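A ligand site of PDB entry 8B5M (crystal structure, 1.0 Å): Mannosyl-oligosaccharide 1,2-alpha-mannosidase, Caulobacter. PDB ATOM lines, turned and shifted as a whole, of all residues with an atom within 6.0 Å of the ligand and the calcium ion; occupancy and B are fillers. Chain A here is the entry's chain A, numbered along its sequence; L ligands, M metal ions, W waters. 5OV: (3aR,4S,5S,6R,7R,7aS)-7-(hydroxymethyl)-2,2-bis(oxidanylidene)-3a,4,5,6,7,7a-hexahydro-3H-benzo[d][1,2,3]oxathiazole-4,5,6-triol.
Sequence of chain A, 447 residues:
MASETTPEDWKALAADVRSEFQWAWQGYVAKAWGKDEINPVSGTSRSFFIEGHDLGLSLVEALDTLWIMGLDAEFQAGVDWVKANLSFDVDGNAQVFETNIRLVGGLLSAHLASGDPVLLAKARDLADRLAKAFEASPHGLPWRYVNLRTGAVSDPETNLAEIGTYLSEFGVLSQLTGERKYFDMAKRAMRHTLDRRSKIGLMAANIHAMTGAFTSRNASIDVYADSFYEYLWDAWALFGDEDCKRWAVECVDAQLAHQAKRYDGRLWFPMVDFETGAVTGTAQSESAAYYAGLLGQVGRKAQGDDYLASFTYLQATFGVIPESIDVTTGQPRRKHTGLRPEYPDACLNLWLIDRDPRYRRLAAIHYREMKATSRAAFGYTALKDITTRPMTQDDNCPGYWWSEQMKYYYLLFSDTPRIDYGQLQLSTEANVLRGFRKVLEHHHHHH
Ile 101 touches the ligand. Pro 341 touches the ligand (CD to O4, 3.6 Å). CD2 of Tyr 400 touches C3 of the ligand (3.6 Å). Hydrophobic or aromatic side chains that line the ligand: Ile 101, Pro 341 and Tyr 400. Within 4 Å of the ligand: Ile 101, Asp 226, Ser 287, Arg 340, Pro 341, Glu 342, Tyr 400, Glu 404, Thr 428 and Glu 429.
The side-chain carboxylate of Glu 230 sits close to the side-chain hydroxyl of Thr 428. OE1 of Glu 404 lies within hydrogen-bond range of OH of Tyr 408 (2.6 Å). The side-chain carboxylate (OE2) of Glu 286 lies within hydrogen-bond range of the backbone NH (N) of Glu 342, at 3.5 Å. The side-chain carboxylate of Glu 429 is in salt-bridge range of the guanidinium group of Arg 102, at 3.9 Å. The backbone NH of Glu 429 lies within hydrogen-bond range of the side-chain hydroxyl of Ser 427, at 3.1 Å. The side-chain hydroxyl (OH) of Tyr 400 sits close to the guanidinium group (NH1) of Arg 340 (3.2 Å). The side-chain hydroxyl of Ser 287 is in hydrogen-bond range of the side-chain hydroxyl of Ser 285 (2.7 Å). The side-chain hydroxyl (OH) of Tyr 400 sits at hydrogen-bond distance from the backbone carbonyl oxygen (O) of Gly 338 (2.6 Å).
The side-chain carboxylate of Glu 404 sits close to an oxygen (O6) of the ligand (2.6 Å). O4 of the ligand sits at hydrogen-bond distance from OE2 of Glu 342. OE1 of Glu 429 lies within hydrogen-bond range of O5 of the ligand (2.7 Å). NH1 of Arg 340 is in hydrogen-bond range of O4 of the ligand (2.8 Å). The side-chain carboxylate of Asp 226 is in hydrogen-bond range of a nitrogen (N1) of the ligand, 3.0 Å away. An oxygen (O2) of the ligand lies close to the side-chain hydroxyl (OG) of Ser 287, at 3.1 Å.
The calcium ion is bound by water W5, water W1, water W8, O7 of the ligand, O6 of the ligand, O of Thr 428, OG1 of Thr 428 and water W3. The calcium ion has eight donor atoms within binding distance.
Water W8 bridges OE1 of Glu 404 (2.7 Å) and OD2 of Asp 345 (2.8 Å). Water W2 lies within hydrogen-bond range of the side-chain hydroxyl of Ser 227 (2.7 Å), the side-chain carboxylate of Asp 226 (2.9 Å) and a nitrogen (N1) of the ligand (3.2 Å). Water W9 lies within hydrogen-bond range of O5 of the ligand (2.8 Å), OE1 of Glu 98 (2.8 Å) and NH2 of Arg 102 (3.3 Å). Water W6 lies within hydrogen-bond range of O2 of the ligand (2.8 Å) and OG of Ser 287 (3.5 Å). Water W4 lies within hydrogen-bond range of the side-chain hydroxyl (OG) of Ser 287 (2.7 Å), the side-chain carboxylate (OD2) of Asp 226 (2.8 Å) and an oxygen (O2) of the ligand (3.2 Å). Water W10 lies within hydrogen-bond range of OD1 of Asp 226 (2.8 Å) and O1 of the ligand (3.2 Å).
Within 4 Å of the calcium ion: Thr 428.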
ATOM      1  N   PHE A  97      32.538  -5.260  39.333  1.00  0.00           N
ATOM      2  CA  PHE A  97      32.216  -5.539  37.928  1.00  0.00           C
ATOM      3  C   PHE A  97      31.105  -4.601  37.452  1.00  0.00           C
ATOM      4  O   PHE A  97      31.213  -4.011  36.368  1.00  0.00           O
ATOM      5  CB  PHE A  97      31.746  -6.990  37.855  1.00  0.00           C
ATOM      6  CG  PHE A  97      31.075  -7.381  36.582  1.00  0.00           C
ATOM      7  CD1 PHE A  97      31.762  -7.759  35.443  1.00  0.00           C
ATOM      8  CD2 PHE A  97      29.682  -7.390  36.529  1.00  0.00           C
ATOM      9  CE1 PHE A  97      31.061  -8.142  34.286  1.00  0.00           C
ATOM     10  CE2 PHE A  97      28.997  -7.705  35.365  1.00  0.00           C
ATOM     11  CZ  PHE A  97      29.697  -8.136  34.243  1.00  0.00           C
ATOM     12  N   GLU A  98      30.015  -4.527  38.214  1.00  0.00           N
ATOM     13  CA  GLU A  98      28.857  -3.758  37.779  1.00  0.00           C
ATOM     14  C   GLU A  98      29.252  -2.282  37.703  1.00  0.00           C
ATOM     15  O   GLU A  98      28.816  -1.536  36.801  1.00  0.00           O
ATOM     16  CB  GLU A  98      27.681  -3.937  38.750  1.00  0.00           C
ATOM     17  CG  GLU A  98      27.139  -5.348  38.882  1.00  0.00           C
ATOM     18  CD  GLU A  98      26.419  -5.939  37.704  1.00  0.00           C
ATOM     19  OE1 GLU A  98      26.140  -5.250  36.758  1.00  0.00           O
ATOM     20  OE2 GLU A  98      26.115  -7.161  37.822  1.00  0.00           O
ATOM     21  N   ILE A 101      31.443  -1.665  34.461  1.00  0.00           N
ATOM     22  CA  ILE A 101      30.853  -1.738  33.113  1.00  0.00           C
ATOM     23  C   ILE A 101      29.753  -0.709  32.964  1.00  0.00           C
ATOM     24  O   ILE A 101      29.497  -0.225  31.846  1.00  0.00           O
ATOM     25  CB  ILE A 101      30.399  -3.135  32.703  1.00  0.00           C
ATOM     26  CG1 ILE A 101      29.189  -3.656  33.481  1.00  0.00           C
ATOM     27  CG2 ILE A 101      31.598  -4.098  32.747  1.00  0.00           C
ATOM     28  CD1 ILE A 101      28.629  -4.941  32.940  1.00  0.00           C
ATOM     29  N   ARG A 102      29.055  -0.356  34.037  1.00  0.00           N
ATOM     30  CA  ARG A 102      27.893   0.555  33.958  1.00  0.00           C
ATOM     31  C   ARG A 102      28.345   2.018  34.168  1.00  0.00           C
ATOM     32  O   ARG A 102      27.973   2.886  33.359  1.00  0.00           O
ATOM     33  CB  ARG A 102      26.854   0.200  35.021  1.00  0.00           C
ATOM     34  CG  ARG A 102      26.248  -1.178  34.808  1.00  0.00           C
ATOM     35  CD  ARG A 102      25.377  -1.568  35.961  1.00  0.00           C
ATOM     36  NE  ARG A 102      24.849  -2.907  35.869  1.00  0.00           N
ATOM     37  CZ  ARG A 102      23.594  -3.185  35.588  1.00  0.00           C
ATOM     38  NH1 ARG A 102      22.750  -2.288  35.121  1.00  0.00           N
ATOM     39  NH2 ARG A 102      23.145  -4.419  35.794  1.00  0.00           N
ATOM     40  N   ASP A 226      30.976 -14.920  30.421  1.00  0.00           N
ATOM     41  CA  ASP A 226      30.656 -14.244  29.160  1.00  0.00           C
ATOM     42  C   ASP A 226      31.697 -13.193  28.720  1.00  0.00           C
ATOM     43  O   ASP A 226      32.407 -13.414  27.715  1.00  0.00           O
ATOM     44  CB  ASP A 226      29.220 -13.713  29.224  1.00  0.00           C
ATOM     45  CG  ASP A 226      28.771 -12.875  30.418  1.00  0.00           C
ATOM     46  OD1 ASP A 226      29.619 -12.421  31.214  1.00  0.00           O
ATOM     47  OD2 ASP A 226      27.538 -12.652  30.525  1.00  0.00           O
ATOM     48  N   SER A 227      31.669 -12.019  29.322  1.00  0.00           N
ATOM     49  CA  SER A 227      32.396 -10.887  28.735  1.00  0.00           C
ATOM     50  C   SER A 227      33.928 -10.994  28.837  1.00  0.00           C
ATOM     51  O   SER A 227      34.610 -10.226  28.153  1.00  0.00           O
ATOM     52  CB  SER A 227      31.879  -9.592  29.359  1.00  0.00           C
ATOM     53  OG  SER A 227      31.804  -9.678  30.771  1.00  0.00           O
ATOM     54  N   GLU A 230      34.780 -11.670  25.272  1.00  0.00           N
ATOM     55  CA  GLU A 230      34.666 -10.438  24.467  1.00  0.00           C
ATOM     56  C   GLU A 230      35.850  -9.536  24.682  1.00  0.00           C
ATOM     57  O   GLU A 230      36.373  -8.991  23.715  1.00  0.00           O
ATOM     58  CB  GLU A 230      33.425  -9.644  24.865  1.00  0.00           C
ATOM     59  CG  GLU A 230      32.102 -10.274  24.432  1.00  0.00           C
ATOM     60  CD  GLU A 230      30.984  -9.374  24.920  1.00  0.00           C
ATOM     61  OE1 GLU A 230      30.696  -9.425  26.153  1.00  0.00           O
ATOM     62  OE2 GLU A 230      30.423  -8.583  24.103  1.00  0.00           O
ATOM     63  N   SER A 285      21.774 -19.768  29.200  1.00  0.00           N
ATOM     64  CA  SER A 285      21.160 -18.467  29.467  1.00  0.00           C
ATOM     65  C   SER A 285      20.780 -17.768  28.156  1.00  0.00           C
ATOM     66  O   SER A 285      21.536 -17.868  27.193  1.00  0.00           O
ATOM     67  CB  SER A 285      22.131 -17.633  30.272  1.00  0.00           C
ATOM     68  OG  SER A 285      21.554 -16.377  30.598  1.00  0.00           O
ATOM     69  N   GLU A 286      19.718 -16.990  28.177  1.00  0.00           N
ATOM     70  CA  GLU A 286      19.457 -16.044  27.081  1.00  0.00           C
ATOM     71  C   GLU A 286      20.717 -15.213  26.811  1.00  0.00           C
ATOM     72  O   GLU A 286      20.990 -14.840  25.675  1.00  0.00           O
ATOM     73  CB  GLU A 286      18.296 -15.140  27.435  1.00  0.00           C
ATOM     74  CG  GLU A 286      17.948 -14.119  26.390  1.00  0.00           C
ATOM     75  CD  GLU A 286      18.852 -12.916  26.319  1.00  0.00           C
ATOM     76  OE1 GLU A 286      19.575 -12.688  27.362  1.00  0.00           O
ATOM     77  OE2 GLU A 286      18.897 -12.190  25.318  1.00  0.00           O
ATOM     78  N   SER A 287      21.448 -14.906  27.888  1.00  0.00           N
ATOM     79  CA  SER A 287      22.565 -13.975  27.804  1.00  0.00           C
ATOM     80  C   SER A 287      23.733 -14.581  27.034  1.00  0.00           C
ATOM     81  O   SER A 287      24.668 -13.843  26.667  1.00  0.00           O
ATOM     82  CB  SER A 287      22.988 -13.502  29.152  1.00  0.00           C
ATOM     83  OG  SER A 287      23.413 -14.589  29.956  1.00  0.00           O
ATOM     84  N   TYR A 290      25.171 -13.164  23.168  1.00  0.00           N
ATOM     85  CA  TYR A 290      26.283 -12.267  22.806  1.00  0.00           C
ATOM     86  C   TYR A 290      27.312 -13.063  21.981  1.00  0.00           C
ATOM     87  O   TYR A 290      28.009 -12.480  21.125  1.00  0.00           O
ATOM     88  CB  TYR A 290      27.004 -11.659  24.037  1.00  0.00           C
ATOM     89  CG  TYR A 290      28.012 -12.613  24.654  1.00  0.00           C
ATOM     90  CD1 TYR A 290      27.607 -13.653  25.466  1.00  0.00           C
ATOM     91  CD2 TYR A 290      29.366 -12.544  24.310  1.00  0.00           C
ATOM     92  CE1 TYR A 290      28.477 -14.637  25.872  1.00  0.00           C
ATOM     93  CE2 TYR A 290      30.257 -13.530  24.708  1.00  0.00           C
ATOM     94  CZ  TYR A 290      29.810 -14.581  25.494  1.00  0.00           C
ATOM     95  OH  TYR A 290      30.707 -15.547  25.842  1.00  0.00           O
ATOM     96  N   GLY A 338      14.620 -10.704  32.357  1.00  0.00           N
ATOM     97  CA  GLY A 338      15.309  -9.487  32.709  1.00  0.00           C
ATOM     98  C   GLY A 338      15.298  -8.429  31.617  1.00  0.00           C
ATOM     99  O   GLY A 338      16.222  -7.581  31.615  1.00  0.00           O
ATOM    100  N   ARG A 340      16.128  -8.511  28.462  1.00  0.00           N
ATOM    101  CA  ARG A 340      17.551  -8.719  28.138  1.00  0.00           C
ATOM    102  C   ARG A 340      17.916  -8.294  26.731  1.00  0.00           C
ATOM    103  O   ARG A 340      17.144  -8.478  25.771  1.00  0.00           O
ATOM    104  CB  ARG A 340      17.875 -10.189  28.325  1.00  0.00           C
ATOM    105  CG  ARG A 340      17.805 -10.693  29.760  1.00  0.00           C
ATOM    106  CD  ARG A 340      19.022 -10.246  30.604  1.00  0.00           C
ATOM    107  NE  ARG A 340      18.840 -10.684  31.968  1.00  0.00           N
ATOM    108  CZ  ARG A 340      19.635 -10.345  32.980  1.00  0.00           C
ATOM    109  NH1 ARG A 340      20.742  -9.633  32.752  1.00  0.00           N
ATOM    110  NH2 ARG A 340      19.356 -10.716  34.235  1.00  0.00           N
ATOM    111  N   PRO A 341      19.154  -7.816  26.546  1.00  0.00           N
ATOM    112  CA  PRO A 341      19.596  -7.195  25.297  1.00  0.00           C
ATOM    113  C   PRO A 341      20.400  -8.054  24.333  1.00  0.00           C
ATOM    114  O   PRO A 341      20.792  -7.537  23.282  1.00  0.00           O
ATOM    115  CB  PRO A 341      20.446  -6.023  25.816  1.00  0.00           C
ATOM    116  CG  PRO A 341      21.166  -6.655  26.966  1.00  0.00           C
ATOM    117  CD  PRO A 341      20.061  -7.419  27.664  1.00  0.00           C
ATOM    118  N   GLU A 342      20.720  -9.312  24.689  1.00  0.00           N
ATOM    119  CA  GLU A 342      21.803  -9.991  23.959  1.00  0.00           C
ATOM    120  C   GLU A 342      21.433 -10.374  22.544  1.00  0.00           C
ATOM    121  O   GLU A 342      22.351 -10.556  21.731  1.00  0.00           O
ATOM    122  CB  GLU A 342      22.336 -11.169  24.731  1.00  0.00           C
ATOM    123  CG  GLU A 342      23.116 -10.784  25.990  1.00  0.00           C
ATOM    124  CD  GLU A 342      22.320 -10.456  27.221  1.00  0.00           C
ATOM    125  OE1 GLU A 342      21.056 -10.581  27.211  1.00  0.00           O
ATOM    126  OE2 GLU A 342      22.954 -10.089  28.243  1.00  0.00           O
ATOM    127  N   ASP A 345      22.178  -7.378  20.425  1.00  0.00           N
ATOM    128  CA  ASP A 345      23.653  -7.281  20.537  1.00  0.00           C
ATOM    129  C   ASP A 345      24.273  -8.137  19.427  1.00  0.00           C
ATOM    130  O   ASP A 345      25.052  -7.618  18.584  1.00  0.00           O
ATOM    131  CB  ASP A 345      24.033  -7.785  21.927  1.00  0.00           C
ATOM    132  CG  ASP A 345      25.497  -7.868  22.224  1.00  0.00           C
ATOM    133  OD1 ASP A 345      26.336  -7.860  21.306  1.00  0.00           O
ATOM    134  OD2 ASP A 345      25.812  -8.055  23.438  1.00  0.00           O
ATOM    135  N   TYR A 400      20.771  -1.542  32.263  1.00  0.00           N
ATOM    136  CA  TYR A 400      21.382  -1.887  30.981  1.00  0.00           C
ATOM    137  C   TYR A 400      20.440  -1.609  29.808  1.00  0.00           C
ATOM    138  O   TYR A 400      20.946  -1.406  28.700  1.00  0.00           O
ATOM    139  CB  TYR A 400      21.915  -3.315  30.934  1.00  0.00           C
ATOM    140  CG  TYR A 400      20.973  -4.401  31.429  1.00  0.00           C
ATOM    141  CD1 TYR A 400      19.879  -4.815  30.698  1.00  0.00           C
ATOM    142  CD2 TYR A 400      21.228  -5.043  32.635  1.00  0.00           C
ATOM    143  CE1 TYR A 400      19.045  -5.838  31.141  1.00  0.00           C
ATOM    144  CE2 TYR A 400      20.395  -6.033  33.104  1.00  0.00           C
ATOM    145  CZ  TYR A 400      19.299  -6.442  32.365  1.00  0.00           C
ATOM    146  OH  TYR A 400      18.476  -7.415  32.873  1.00  0.00           O
ATOM    147  N   GLU A 404      21.912  -0.450  26.225  1.00  0.00           N
ATOM    148  CA  GLU A 404      22.038  -1.563  25.275  1.00  0.00           C
ATOM    149  C   GLU A 404      20.955  -1.607  24.194  1.00  0.00           C
ATOM    150  O   GLU A 404      21.209  -1.180  23.078  1.00  0.00           O
ATOM    151  CB  GLU A 404      22.157  -2.886  26.012  1.00  0.00           C
ATOM    152  CG  GLU A 404      23.389  -2.929  26.910  1.00  0.00           C
ATOM    153  CD  GLU A 404      23.879  -4.346  27.113  1.00  0.00           C
ATOM    154  OE1 GLU A 404      23.998  -5.099  26.113  1.00  0.00           O
ATOM    155  OE2 GLU A 404      24.149  -4.674  28.300  1.00  0.00           O
ATOM    156  N   TYR A 408      21.243  -0.588  20.292  1.00  0.00           N
ATOM    157  CA  TYR A 408      21.452  -1.587  19.251  1.00  0.00           C
ATOM    158  C   TYR A 408      20.460  -1.421  18.101  1.00  0.00           C
ATOM    159  O   TYR A 408      20.822  -1.400  16.921  1.00  0.00           O
ATOM    160  CB  TYR A 408      21.380  -3.033  19.764  1.00  0.00           C
ATOM    161  CG  TYR A 408      22.384  -3.398  20.829  1.00  0.00           C
ATOM    162  CD1 TYR A 408      23.685  -2.931  20.826  1.00  0.00           C
ATOM    163  CD2 TYR A 408      21.993  -4.271  21.818  1.00  0.00           C
ATOM    164  CE1 TYR A 408      24.585  -3.333  21.816  1.00  0.00           C
ATOM    165  CE2 TYR A 408      22.878  -4.656  22.832  1.00  0.00           C
ATOM    166  CZ  TYR A 408      24.172  -4.164  22.843  1.00  0.00           C
ATOM    167  OH  TYR A 408      25.050  -4.508  23.844  1.00  0.00           O
ATOM    168  N   SER A 427      31.446  -1.567  24.329  1.00  0.00           N
ATOM    169  CA  SER A 427      31.733  -2.354  25.514  1.00  0.00           C
ATOM    170  C   SER A 427      30.666  -3.432  25.696  1.00  0.00           C
ATOM    171  O   SER A 427      29.686  -3.484  24.936  1.00  0.00           O
ATOM    172  CB  SER A 427      31.824  -1.466  26.749  1.00  0.00           C
ATOM    173  OG  SER A 427      30.499  -1.243  27.266  1.00  0.00           O
ATOM    174  N   THR A 428      30.833  -4.278  26.710  1.00  0.00           N
ATOM    175  CA  THR A 428      29.824  -5.326  26.933  1.00  0.00           C
ATOM    176  C   THR A 428      28.501  -4.751  27.441  1.00  0.00           C
ATOM    177  O   THR A 428      27.510  -5.482  27.450  1.00  0.00           O
ATOM    178  CB  THR A 428      30.350  -6.428  27.859  1.00  0.00           C
ATOM    179  OG1 THR A 428      29.552  -7.604  27.689  1.00  0.00           O
ATOM    180  CG2 THR A 428      30.351  -6.050  29.335  1.00  0.00           C
ATOM    181  N   GLU A 429      28.522  -3.489  27.873  1.00  0.00           N
ATOM    182  CA  GLU A 429      27.340  -2.726  28.295  1.00  0.00           C
ATOM    183  C   GLU A 429      26.900  -1.776  27.178  1.00  0.00           C
ATOM    184  O   GLU A 429      26.108  -0.859  27.417  1.00  0.00           O
ATOM    185  CB  GLU A 429      27.703  -1.961  29.579  1.00  0.00           C
ATOM    186  CG  GLU A 429      26.547  -1.364  30.329  1.00  0.00           C
ATOM    187  CD  GLU A 429      25.762  -2.345  31.144  1.00  0.00           C
ATOM    188  OE1 GLU A 429      26.111  -3.533  31.224  1.00  0.00           O
ATOM    189  OE2 GLU A 429      24.712  -1.924  31.778  1.00  0.00           O
HETATM  190  C1  5OV L   1      25.519  -8.997  30.935  1.00  0.00           C
HETATM  191  C2  5OV L   1      24.504  -8.578  31.948  1.00  0.00           C
HETATM  192  C3  5OV L   1      23.622  -7.460  31.446  1.00  0.00           C
HETATM  193  C4  5OV L   1      22.745  -7.721  30.232  1.00  0.00           C
HETATM  194  C5  5OV L   1      24.560  -6.287  31.154  1.00  0.00           C
HETATM  195  C6  5OV L   1      25.785  -6.631  30.291  1.00  0.00           C
HETATM  196  C7  5OV L   1      26.528  -7.870  30.782  1.00  0.00           C
HETATM  197  N1  5OV L   1      26.064 -10.245  31.521  1.00  0.00           N
HETATM  198  O1  5OV L   1      25.255 -11.368  33.578  1.00  0.00           O
HETATM  199  S1  5OV L   1      24.854 -11.000  32.270  1.00  0.00           S
HETATM  200  O2  5OV L   1      24.268 -12.050  31.513  1.00  0.00           O
HETATM  201  O3  5OV L   1      23.838  -9.807  32.320  1.00  0.00           O
HETATM  202  O4  5OV L   1      21.901  -8.865  30.357  1.00  0.00           O
HETATM  203  O5  5OV L   1      24.966  -5.700  32.399  1.00  0.00           O
HETATM  204  O6  5OV L   1      25.418  -6.891  28.933  1.00  0.00           O
HETATM  205  O7  5OV L   1      27.550  -8.150  29.820  1.00  0.00           O
HETATM  206 CA    CA M   1      27.087  -7.939  27.435  1.00  0.00          CA
HETATM  207  O   HOH W   1      27.915  -7.958  25.173  1.00  0.00           O
HETATM  208  O   HOH W   2      29.199  -9.598  31.343  1.00  0.00           O
HETATM  209  O   HOH W   3      28.347 -10.177  27.428  1.00  0.00           O
HETATM  210  O   HOH W   4      25.826 -14.794  31.219  1.00  0.00           O
HETATM  211  O   HOH W   5      25.611  -9.764  27.784  1.00  0.00           O
HETATM  212  O   HOH W   6      22.053 -13.232  32.843  1.00  0.00           O
HETATM  213  O   HOH W   7      22.460  -8.494  35.043  1.00  0.00           O
HETATM  214  O   HOH W   8      25.116  -7.515  26.071  1.00  0.00           O
HETATM  215  O   HOH W   9      25.050  -6.996  34.830  1.00  0.00           O
HETATM  216  O   HOH W  10      28.361 -12.205  33.732  1.00  0.00           O
HETATM  217  O   HOH W  11      25.720  -9.356  36.101  1.00  0.00           O
